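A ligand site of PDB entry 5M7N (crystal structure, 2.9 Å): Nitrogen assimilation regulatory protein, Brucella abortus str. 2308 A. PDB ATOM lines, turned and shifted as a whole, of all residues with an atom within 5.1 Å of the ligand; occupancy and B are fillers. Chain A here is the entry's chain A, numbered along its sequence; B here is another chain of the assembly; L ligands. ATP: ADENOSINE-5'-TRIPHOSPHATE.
An oxygen (O1G) of the ligand lies within salt-bridge range of the guanidinium group (NE) of Arg 357.
N of Val 144 lies within hydrogen-bond range of N1 of the ligand (2.8 Å).
O of Val 144 is in hydrogen-bond range of N6 of the ligand (3.1 Å).
O1G of the ligand lies within salt-bridge range of NH2 of Arg 371 of chain B (2.8 Å).
An oxygen (O1B) of the ligand sits at hydrogen-bond distance from the backbone NH of Lys 177 (2.9 Å).
NZ of Lys 177 is in salt-bridge range of O1B of the ligand, 3.1 Å away.
The backbone NH (N) of Glu 178 is in hydrogen-bond range of an oxygen (O2B) of the ligand (3.0 Å).
O1B of the ligand sits at hydrogen-bond distance from N of Gly 176 (3.0 Å).
O3B of the ligand is in hydrogen-bond range of N of Gly 174 (3.0 Å).
O of Ala 332 of chain B lies close to O3G of the ligand (3.1 Å).
O1A of the ligand sits at hydrogen-bond distance from N of Leu 179 (3.1 Å).
N of Ala 175 sits at hydrogen-bond distance from O1B of the ligand (3.3 Å).
The backbone NH (N) of Arg 357 sits at hydrogen-bond distance from the backbone carbonyl oxygen (O) of Gly 174 (3.2 Å).
The side-chain amino group of Lys 177 is in hydrogen-bond range of the backbone carbonyl oxygen of Pro 172.
OH of Tyr 236 is in hydrogen-bond range of N of Glu 178 (3.3 Å).
The backbone carbonyl oxygen (O) of Gly 174 sits at hydrogen-bond distance from the backbone NH (N) of Leu 356.
The backbone carbonyl oxygen of Ala 175 is in hydrogen-bond range of the guanidinium group of Arg 313 (2.8 Å).
The guanidinium group (NH1) of Arg 313 sits at hydrogen-bond distance from the side-chain sulfur (SD) of Met 150, at 3.5 Å.
Residues that only touch the ligand: Leu 356, Met 150, Leu 320, Leu 143, Arg 313, Arg 360, Pro 172 and Glu 142.
Hydrophobic or aromatic side chains that line the ligand: Leu 143, Val 144, Met 150, Leu 179, Leu 320 and Leu 356.
18 residues have an atom within 4 Å of the ligand: Glu 142, Leu 143, Val 144, Met 150, Pro 172, Gly 174, Ala 175, Gly 176, Lys 177, Glu 178, Leu 179, Arg 313, Leu 320, Leu 356, Arg 357, Arg 360, Ala 332 of chain B and Arg 371 of chain B.
The nearest printed residue that does not touch the ligand is Phe 323 (4.04 Å).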
ATOM      1  N   GLU A 142      35.433  22.148  27.442  1.00  0.00           N
ATOM      2  CA  GLU A 142      36.242  23.109  28.178  1.00  0.00           C
ATOM      3  C   GLU A 142      35.990  24.531  27.694  1.00  0.00           C
ATOM      4  O   GLU A 142      35.624  24.770  26.533  1.00  0.00           O
ATOM      5  CB  GLU A 142      37.761  22.743  28.101  1.00  0.00           C
ATOM      6  CG  GLU A 142      38.716  23.598  28.948  1.00  0.00           C
ATOM      7  CD  GLU A 142      38.538  23.583  30.455  1.00  0.00           C
ATOM      8  OE1 GLU A 142      38.739  22.503  31.066  1.00  0.00           O
ATOM      9  OE2 GLU A 142      38.262  24.654  31.034  1.00  0.00           O
ATOM     10  N   LEU A 143      36.175  25.473  28.626  1.00  0.00           N
ATOM     11  CA  LEU A 143      36.041  26.895  28.407  1.00  0.00           C
ATOM     12  C   LEU A 143      37.435  27.438  28.136  1.00  0.00           C
ATOM     13  O   LEU A 143      38.310  27.365  28.991  1.00  0.00           O
ATOM     14  CB  LEU A 143      35.437  27.546  29.659  1.00  0.00           C
ATOM     15  CG  LEU A 143      34.007  27.164  30.019  1.00  0.00           C
ATOM     16  CD1 LEU A 143      33.715  27.573  31.412  1.00  0.00           C
ATOM     17  CD2 LEU A 143      32.987  27.818  29.074  1.00  0.00           C
ATOM     18  N   VAL A 144      37.648  27.887  26.900  1.00  0.00           N
ATOM     19  CA  VAL A 144      38.890  28.473  26.393  1.00  0.00           C
ATOM     20  C   VAL A 144      38.959  29.963  26.797  1.00  0.00           C
ATOM     21  O   VAL A 144      37.954  30.682  26.789  1.00  0.00           O
ATOM     22  CB  VAL A 144      39.046  28.240  24.857  1.00  0.00           C
ATOM     23  CG1 VAL A 144      40.356  28.804  24.335  1.00  0.00           C
ATOM     24  CG2 VAL A 144      38.962  26.764  24.519  1.00  0.00           C
ATOM     25  N   MET A 150      38.126  34.884  32.463  1.00  0.00           N
ATOM     26  CA  MET A 150      37.904  33.459  32.252  1.00  0.00           C
ATOM     27  C   MET A 150      38.332  32.609  33.438  1.00  0.00           C
ATOM     28  O   MET A 150      37.552  31.743  33.860  1.00  0.00           O
ATOM     29  CB  MET A 150      38.532  32.970  30.953  1.00  0.00           C
ATOM     30  CG  MET A 150      37.649  33.239  29.763  1.00  0.00           C
ATOM     31  SD  MET A 150      35.910  32.805  30.030  1.00  0.00           S
ATOM     32  CE  MET A 150      36.033  31.008  30.161  1.00  0.00           C
ATOM     33  N   PRO A 172      25.319  37.984  27.839  1.00  0.00           N
ATOM     34  CA  PRO A 172      24.746  38.222  26.496  1.00  0.00           C
ATOM     35  C   PRO A 172      24.615  36.956  25.641  1.00  0.00           C
ATOM     36  O   PRO A 172      25.105  35.886  26.015  1.00  0.00           O
ATOM     37  CB  PRO A 172      25.749  39.200  25.878  1.00  0.00           C
ATOM     38  CG  PRO A 172      27.014  38.947  26.605  1.00  0.00           C
ATOM     39  CD  PRO A 172      26.590  38.704  28.001  1.00  0.00           C
ATOM     40  N   SER A 173      23.974  37.085  24.476  1.00  0.00           N
ATOM     41  CA  SER A 173      23.753  35.981  23.525  1.00  0.00           C
ATOM     42  C   SER A 173      25.056  35.355  22.999  1.00  0.00           C
ATOM     43  O   SER A 173      25.963  36.078  22.565  1.00  0.00           O
ATOM     44  CB  SER A 173      22.876  36.453  22.378  1.00  0.00           C
ATOM     45  OG  SER A 173      21.643  36.960  22.860  1.00  0.00           O
ATOM     46  N   GLY A 174      25.127  34.022  23.072  1.00  0.00           N
ATOM     47  CA  GLY A 174      26.249  33.197  22.626  1.00  0.00           C
ATOM     48  C   GLY A 174      27.559  33.402  23.378  1.00  0.00           C
ATOM     49  O   GLY A 174      28.615  33.178  22.797  1.00  0.00           O
ATOM     50  N   ALA A 175      27.494  33.807  24.675  1.00  0.00           N
ATOM     51  CA  ALA A 175      28.669  34.056  25.516  1.00  0.00           C
ATOM     52  C   ALA A 175      29.212  32.814  26.232  1.00  0.00           C
ATOM     53  O   ALA A 175      30.347  32.843  26.730  1.00  0.00           O
ATOM     54  CB  ALA A 175      28.363  35.150  26.525  1.00  0.00           C
ATOM     55  N   GLY A 176      28.397  31.763  26.324  1.00  0.00           N
ATOM     56  CA  GLY A 176      28.786  30.511  26.962  1.00  0.00           C
ATOM     57  C   GLY A 176      28.084  30.158  28.254  1.00  0.00           C
ATOM     58  O   GLY A 176      28.635  29.386  29.041  1.00  0.00           O
ATOM     59  N   LYS A 177      26.862  30.691  28.475  1.00  0.00           N
ATOM     60  CA  LYS A 177      26.032  30.423  29.669  1.00  0.00           C
ATOM     61  C   LYS A 177      25.636  28.951  29.768  1.00  0.00           C
ATOM     62  O   LYS A 177      25.641  28.402  30.859  1.00  0.00           O
ATOM     63  CB  LYS A 177      24.750  31.267  29.660  1.00  0.00           C
ATOM     64  CG  LYS A 177      24.947  32.772  29.606  1.00  0.00           C
ATOM     65  CD  LYS A 177      23.623  33.506  29.684  1.00  0.00           C
ATOM     66  CE  LYS A 177      22.753  33.343  28.474  1.00  0.00           C
ATOM     67  NZ  LYS A 177      23.290  34.027  27.294  1.00  0.00           N
ATOM     68  N   GLU A 178      25.278  28.328  28.636  1.00  0.00           N
ATOM     69  CA  GLU A 178      24.908  26.913  28.581  1.00  0.00           C
ATOM     70  C   GLU A 178      26.116  26.060  28.918  1.00  0.00           C
ATOM     71  O   GLU A 178      25.978  25.101  29.677  1.00  0.00           O
ATOM     72  CB  GLU A 178      24.409  26.564  27.174  1.00  0.00           C
ATOM     73  CG  GLU A 178      23.906  25.151  26.966  1.00  0.00           C
ATOM     74  CD  GLU A 178      23.022  25.005  25.750  1.00  0.00           C
ATOM     75  OE1 GLU A 178      22.836  26.003  25.000  1.00  0.00           O
ATOM     76  OE2 GLU A 178      22.480  23.889  25.563  1.00  0.00           O
ATOM     77  N   LEU A 179      27.291  26.434  28.368  1.00  0.00           N
ATOM     78  CA  LEU A 179      28.544  25.744  28.632  1.00  0.00           C
ATOM     79  C   LEU A 179      28.873  25.778  30.127  1.00  0.00           C
ATOM     80  O   LEU A 179      29.144  24.728  30.679  1.00  0.00           O
ATOM     81  CB  LEU A 179      29.681  26.294  27.778  1.00  0.00           C
ATOM     82  CG  LEU A 179      30.461  25.212  27.035  1.00  0.00           C
ATOM     83  CD1 LEU A 179      29.682  24.715  25.798  1.00  0.00           C
ATOM     84  CD2 LEU A 179      31.825  25.689  26.636  1.00  0.00           C
ATOM     85  N   TYR A 236      18.043  22.877  33.219  1.00  0.00           N
ATOM     86  CA  TYR A 236      18.601  24.110  32.712  1.00  0.00           C
ATOM     87  C   TYR A 236      17.511  24.859  32.022  1.00  0.00           C
ATOM     88  O   TYR A 236      17.038  24.420  30.973  1.00  0.00           O
ATOM     89  CB  TYR A 236      19.794  23.878  31.780  1.00  0.00           C
ATOM     90  CG  TYR A 236      20.414  25.153  31.258  1.00  0.00           C
ATOM     91  CD1 TYR A 236      20.895  26.127  32.129  1.00  0.00           C
ATOM     92  CD2 TYR A 236      20.533  25.384  29.888  1.00  0.00           C
ATOM     93  CE1 TYR A 236      21.473  27.301  31.659  1.00  0.00           C
ATOM     94  CE2 TYR A 236      21.140  26.546  29.405  1.00  0.00           C
ATOM     95  CZ  TYR A 236      21.605  27.504  30.287  1.00  0.00           C
ATOM     96  OH  TYR A 236      22.175  28.660  29.807  1.00  0.00           O
ATOM     97  N   ASP A 238      16.856  27.753  30.051  1.00  0.00           N
ATOM     98  CA  ASP A 238      17.471  28.666  29.083  1.00  0.00           C
ATOM     99  C   ASP A 238      16.466  29.747  28.750  1.00  0.00           C
ATOM    100  O   ASP A 238      15.444  29.475  28.118  1.00  0.00           O
ATOM    101  CB  ASP A 238      17.902  27.906  27.810  1.00  0.00           C
ATOM    102  CG  ASP A 238      18.814  28.683  26.867  1.00  0.00           C
ATOM    103  OD1 ASP A 238      19.712  29.410  27.359  1.00  0.00           O
ATOM    104  OD2 ASP A 238      18.689  28.487  25.633  1.00  0.00           O
ATOM    105  N   ARG A 313      36.455  40.717  26.895  1.00  0.00           N
ATOM    106  CA  ARG A 313      37.545  39.733  27.028  1.00  0.00           C
ATOM    107  C   ARG A 313      38.231  39.459  25.679  1.00  0.00           C
ATOM    108  O   ARG A 313      38.532  38.318  25.331  1.00  0.00           O
ATOM    109  CB  ARG A 313      37.072  38.430  27.687  1.00  0.00           C
ATOM    110  CG  ARG A 313      35.823  37.868  27.053  1.00  0.00           C
ATOM    111  CD  ARG A 313      35.633  36.443  27.449  1.00  0.00           C
ATOM    112  NE  ARG A 313      34.220  36.086  27.355  1.00  0.00           N
ATOM    113  CZ  ARG A 313      33.770  34.853  27.142  1.00  0.00           C
ATOM    114  NH1 ARG A 313      34.636  33.853  26.988  1.00  0.00           N
ATOM    115  NH2 ARG A 313      32.477  34.613  27.078  1.00  0.00           N
ATOM    116  N   LEU A 320      40.675  31.668  20.894  1.00  0.00           N
ATOM    117  CA  LEU A 320      39.362  31.148  20.524  1.00  0.00           C
ATOM    118  C   LEU A 320      39.309  30.848  19.069  1.00  0.00           C
ATOM    119  O   LEU A 320      38.766  29.824  18.701  1.00  0.00           O
ATOM    120  CB  LEU A 320      38.231  32.091  20.948  1.00  0.00           C
ATOM    121  CG  LEU A 320      37.983  32.235  22.461  1.00  0.00           C
ATOM    122  CD1 LEU A 320      37.127  33.439  22.745  1.00  0.00           C
ATOM    123  CD2 LEU A 320      37.385  30.990  23.056  1.00  0.00           C
ATOM    124  N   PHE A 323      41.268  27.722  18.586  1.00  0.00           N
ATOM    125  CA  PHE A 323      40.436  26.674  19.128  1.00  0.00           C
ATOM    126  C   PHE A 323      39.329  26.287  18.154  1.00  0.00           C
ATOM    127  O   PHE A 323      39.127  25.099  17.905  1.00  0.00           O
ATOM    128  CB  PHE A 323      39.847  27.081  20.478  1.00  0.00           C
ATOM    129  CG  PHE A 323      38.866  26.058  21.014  1.00  0.00           C
ATOM    130  CD1 PHE A 323      39.311  24.881  21.583  1.00  0.00           C
ATOM    131  CD2 PHE A 323      37.490  26.279  20.909  1.00  0.00           C
ATOM    132  CE1 PHE A 323      38.405  23.950  22.083  1.00  0.00           C
ATOM    133  CE2 PHE A 323      36.586  25.332  21.406  1.00  0.00           C
ATOM    134  CZ  PHE A 323      37.045  24.178  22.002  1.00  0.00           C
ATOM    135  N   PHE A 324      38.619  27.274  17.621  1.00  0.00           N
ATOM    136  CA  PHE A 324      37.503  27.055  16.712  1.00  0.00           C
ATOM    137  C   PHE A 324      37.975  26.404  15.423  1.00  0.00           C
ATOM    138  O   PHE A 324      37.349  25.458  14.969  1.00  0.00           O
ATOM    139  CB  PHE A 324      36.675  28.345  16.500  1.00  0.00           C
ATOM    140  CG  PHE A 324      35.877  28.798  17.709  1.00  0.00           C
ATOM    141  CD1 PHE A 324      35.163  27.891  18.479  1.00  0.00           C
ATOM    142  CD2 PHE A 324      35.801  30.148  18.048  1.00  0.00           C
ATOM    143  CE1 PHE A 324      34.385  28.326  19.573  1.00  0.00           C
ATOM    144  CE2 PHE A 324      35.055  30.575  19.159  1.00  0.00           C
ATOM    145  CZ  PHE A 324      34.358  29.655  19.908  1.00  0.00           C
ATOM    146  N   LEU A 356      30.672  34.518  21.254  1.00  0.00           N
ATOM    147  CA  LEU A 356      31.367  33.289  20.855  1.00  0.00           C
ATOM    148  C   LEU A 356      30.606  32.439  19.838  1.00  0.00           C
ATOM    149  O   LEU A 356      31.258  31.747  19.060  1.00  0.00           O
ATOM    150  CB  LEU A 356      31.792  32.435  22.069  1.00  0.00           C
ATOM    151  CG  LEU A 356      32.978  33.012  22.841  1.00  0.00           C
ATOM    152  CD1 LEU A 356      32.535  33.931  23.940  1.00  0.00           C
ATOM    153  CD2 LEU A 356      33.797  31.921  23.452  1.00  0.00           C
ATOM    154  N   ARG A 357      29.256  32.518  19.781  1.00  0.00           N
ATOM    155  CA  ARG A 357      28.499  31.782  18.759  1.00  0.00           C
ATOM    156  C   ARG A 357      28.857  32.393  17.389  1.00  0.00           C
ATOM    157  O   ARG A 357      29.322  31.679  16.486  1.00  0.00           O
ATOM    158  CB  ARG A 357      26.982  31.870  19.000  1.00  0.00           C
ATOM    159  CG  ARG A 357      26.140  31.009  18.065  1.00  0.00           C
ATOM    160  CD  ARG A 357      24.773  30.713  18.682  1.00  0.00           C
ATOM    161  NE  ARG A 357      24.838  29.797  19.823  1.00  0.00           N
ATOM    162  CZ  ARG A 357      24.874  28.472  19.720  1.00  0.00           C
ATOM    163  NH1 ARG A 357      24.839  27.879  18.537  1.00  0.00           N
ATOM    164  NH2 ARG A 357      24.920  27.717  20.824  1.00  0.00           N
ATOM    165  N   ARG A 360      32.554  31.866  16.349  1.00  0.00           N
ATOM    166  CA  ARG A 360      32.651  30.490  15.859  1.00  0.00           C
ATOM    167  C   ARG A 360      32.134  30.370  14.431  1.00  0.00           C
ATOM    168  O   ARG A 360      32.836  29.836  13.573  1.00  0.00           O
ATOM    169  CB  ARG A 360      31.876  29.551  16.768  1.00  0.00           C
ATOM    170  CG  ARG A 360      32.344  28.123  16.695  1.00  0.00           C
ATOM    171  CD  ARG A 360      31.211  27.172  16.993  1.00  0.00           C
ATOM    172  NE  ARG A 360      30.507  26.877  15.742  1.00  0.00           N
ATOM    173  CZ  ARG A 360      30.854  25.919  14.899  1.00  0.00           C
ATOM    174  NH1 ARG A 360      31.872  25.098  15.189  1.00  0.00           N
ATOM    175  NH2 ARG A 360      30.175  25.743  13.767  1.00  0.00           N
ATOM    176  N   GLN B 331      19.735  23.903  19.391  1.00  0.00           N
ATOM    177  CA  GLN B 331      21.130  24.119  19.765  1.00  0.00           C
ATOM    178  C   GLN B 331      21.350  25.453  20.510  1.00  0.00           C
ATOM    179  O   GLN B 331      22.014  25.477  21.548  1.00  0.00           O
ATOM    180  CB  GLN B 331      22.007  24.108  18.503  1.00  0.00           C
ATOM    181  CG  GLN B 331      22.266  22.744  17.883  1.00  0.00           C
ATOM    182  CD  GLN B 331      23.300  22.864  16.786  1.00  0.00           C
ATOM    183  OE1 GLN B 331      24.351  23.519  16.949  1.00  0.00           O
ATOM    184  NE2 GLN B 331      23.035  22.233  15.649  1.00  0.00           N
ATOM    185  N   ALA B 332      20.784  26.570  19.976  1.00  0.00           N
ATOM    186  CA  ALA B 332      20.982  27.917  20.469  1.00  0.00           C
ATOM    187  C   ALA B 332      19.770  28.590  21.127  1.00  0.00           C
ATOM    188  O   ALA B 332      19.935  29.647  21.749  1.00  0.00           O
ATOM    189  CB  ALA B 332      21.492  28.791  19.340  1.00  0.00           C
ATOM    190  N   ARG B 371      18.402  37.297  15.329  1.00  0.00           N
ATOM    191  CA  ARG B 371      18.021  36.822  16.656  1.00  0.00           C
ATOM    192  C   ARG B 371      17.245  37.846  17.493  1.00  0.00           C
ATOM    193  O   ARG B 371      16.224  37.493  18.085  1.00  0.00           O
ATOM    194  CB  ARG B 371      19.280  36.326  17.393  1.00  0.00           C
ATOM    195  CG  ARG B 371      18.991  35.527  18.644  1.00  0.00           C
ATOM    196  CD  ARG B 371      19.985  35.891  19.710  1.00  0.00           C
ATOM    197  NE  ARG B 371      21.108  34.951  19.759  1.00  0.00           N
ATOM    198  CZ  ARG B 371      21.134  33.865  20.528  1.00  0.00           C
ATOM    199  NH1 ARG B 371      20.082  33.548  21.273  1.00  0.00           N
ATOM    200  NH2 ARG B 371      22.202  33.079  20.542  1.00  0.00           N
HETATM  201  PG  ATP L   1      23.000  30.922  23.277  1.00  0.00           P
HETATM  202  O1G ATP L   1      23.617  31.125  21.890  1.00  0.00           O
HETATM  203  O2G ATP L   1      22.795  29.421  23.689  1.00  0.00           O
HETATM  204  O3G ATP L   1      21.616  31.585  23.417  1.00  0.00           O
HETATM  205  PB  ATP L   1      24.915  30.927  25.502  1.00  0.00           P
HETATM  206  O1B ATP L   1      25.394  31.997  26.401  1.00  0.00           O
HETATM  207  O2B ATP L   1      24.154  29.865  26.325  1.00  0.00           O
HETATM  208  O3B ATP L   1      23.965  31.553  24.389  1.00  0.00           O
HETATM  209  PA  ATP L   1      26.484  28.673  24.558  1.00  0.00           P
HETATM  210  O1A ATP L   1      27.293  28.066  25.715  1.00  0.00           O
HETATM  211  O2A ATP L   1      25.191  27.961  24.344  1.00  0.00           O
HETATM  212  O3A ATP L   1      26.182  30.208  24.859  1.00  0.00           O
HETATM  213  O5' ATP L   1      27.336  28.600  23.242  1.00  0.00           O
HETATM  214  C5' ATP L   1      28.429  29.472  22.900  1.00  0.00           C
HETATM  215  C4' ATP L   1      29.256  28.808  21.824  1.00  0.00           C
HETATM  216  O4' ATP L   1      30.654  29.088  22.049  1.00  0.00           O
HETATM  217  C3' ATP L   1      29.182  27.287  21.732  1.00  0.00           C
HETATM  218  O3' ATP L   1      29.413  26.867  20.395  1.00  0.00           O
HETATM  219  C2' ATP L   1      30.242  26.839  22.731  1.00  0.00           C
HETATM  220  O2' ATP L   1      30.893  25.634  22.366  1.00  0.00           O
HETATM  221  C1' ATP L   1      31.273  27.971  22.655  1.00  0.00           C
HETATM  222  N9  ATP L   1      31.841  28.391  23.964  1.00  0.00           N
HETATM  223  C8  ATP L   1      31.216  29.116  24.900  1.00  0.00           C
HETATM  224  N7  ATP L   1      32.035  29.589  25.845  1.00  0.00           N
HETATM  225  C5  ATP L   1      33.275  29.086  25.435  1.00  0.00           C
HETATM  226  C6  ATP L   1      34.577  29.338  25.926  1.00  0.00           C
HETATM  227  N6  ATP L   1      34.862  30.117  26.977  1.00  0.00           N
HETATM  228  N1  ATP L   1      35.607  28.755  25.251  1.00  0.00           N
HETATM  229  C2  ATP L   1      35.336  27.978  24.194  1.00  0.00           C
HETATM  230  N3  ATP L   1      34.157  27.700  23.650  1.00  0.00           N
HETATM  231  C4  ATP L   1      33.153  28.310  24.289  1.00  0.00           C
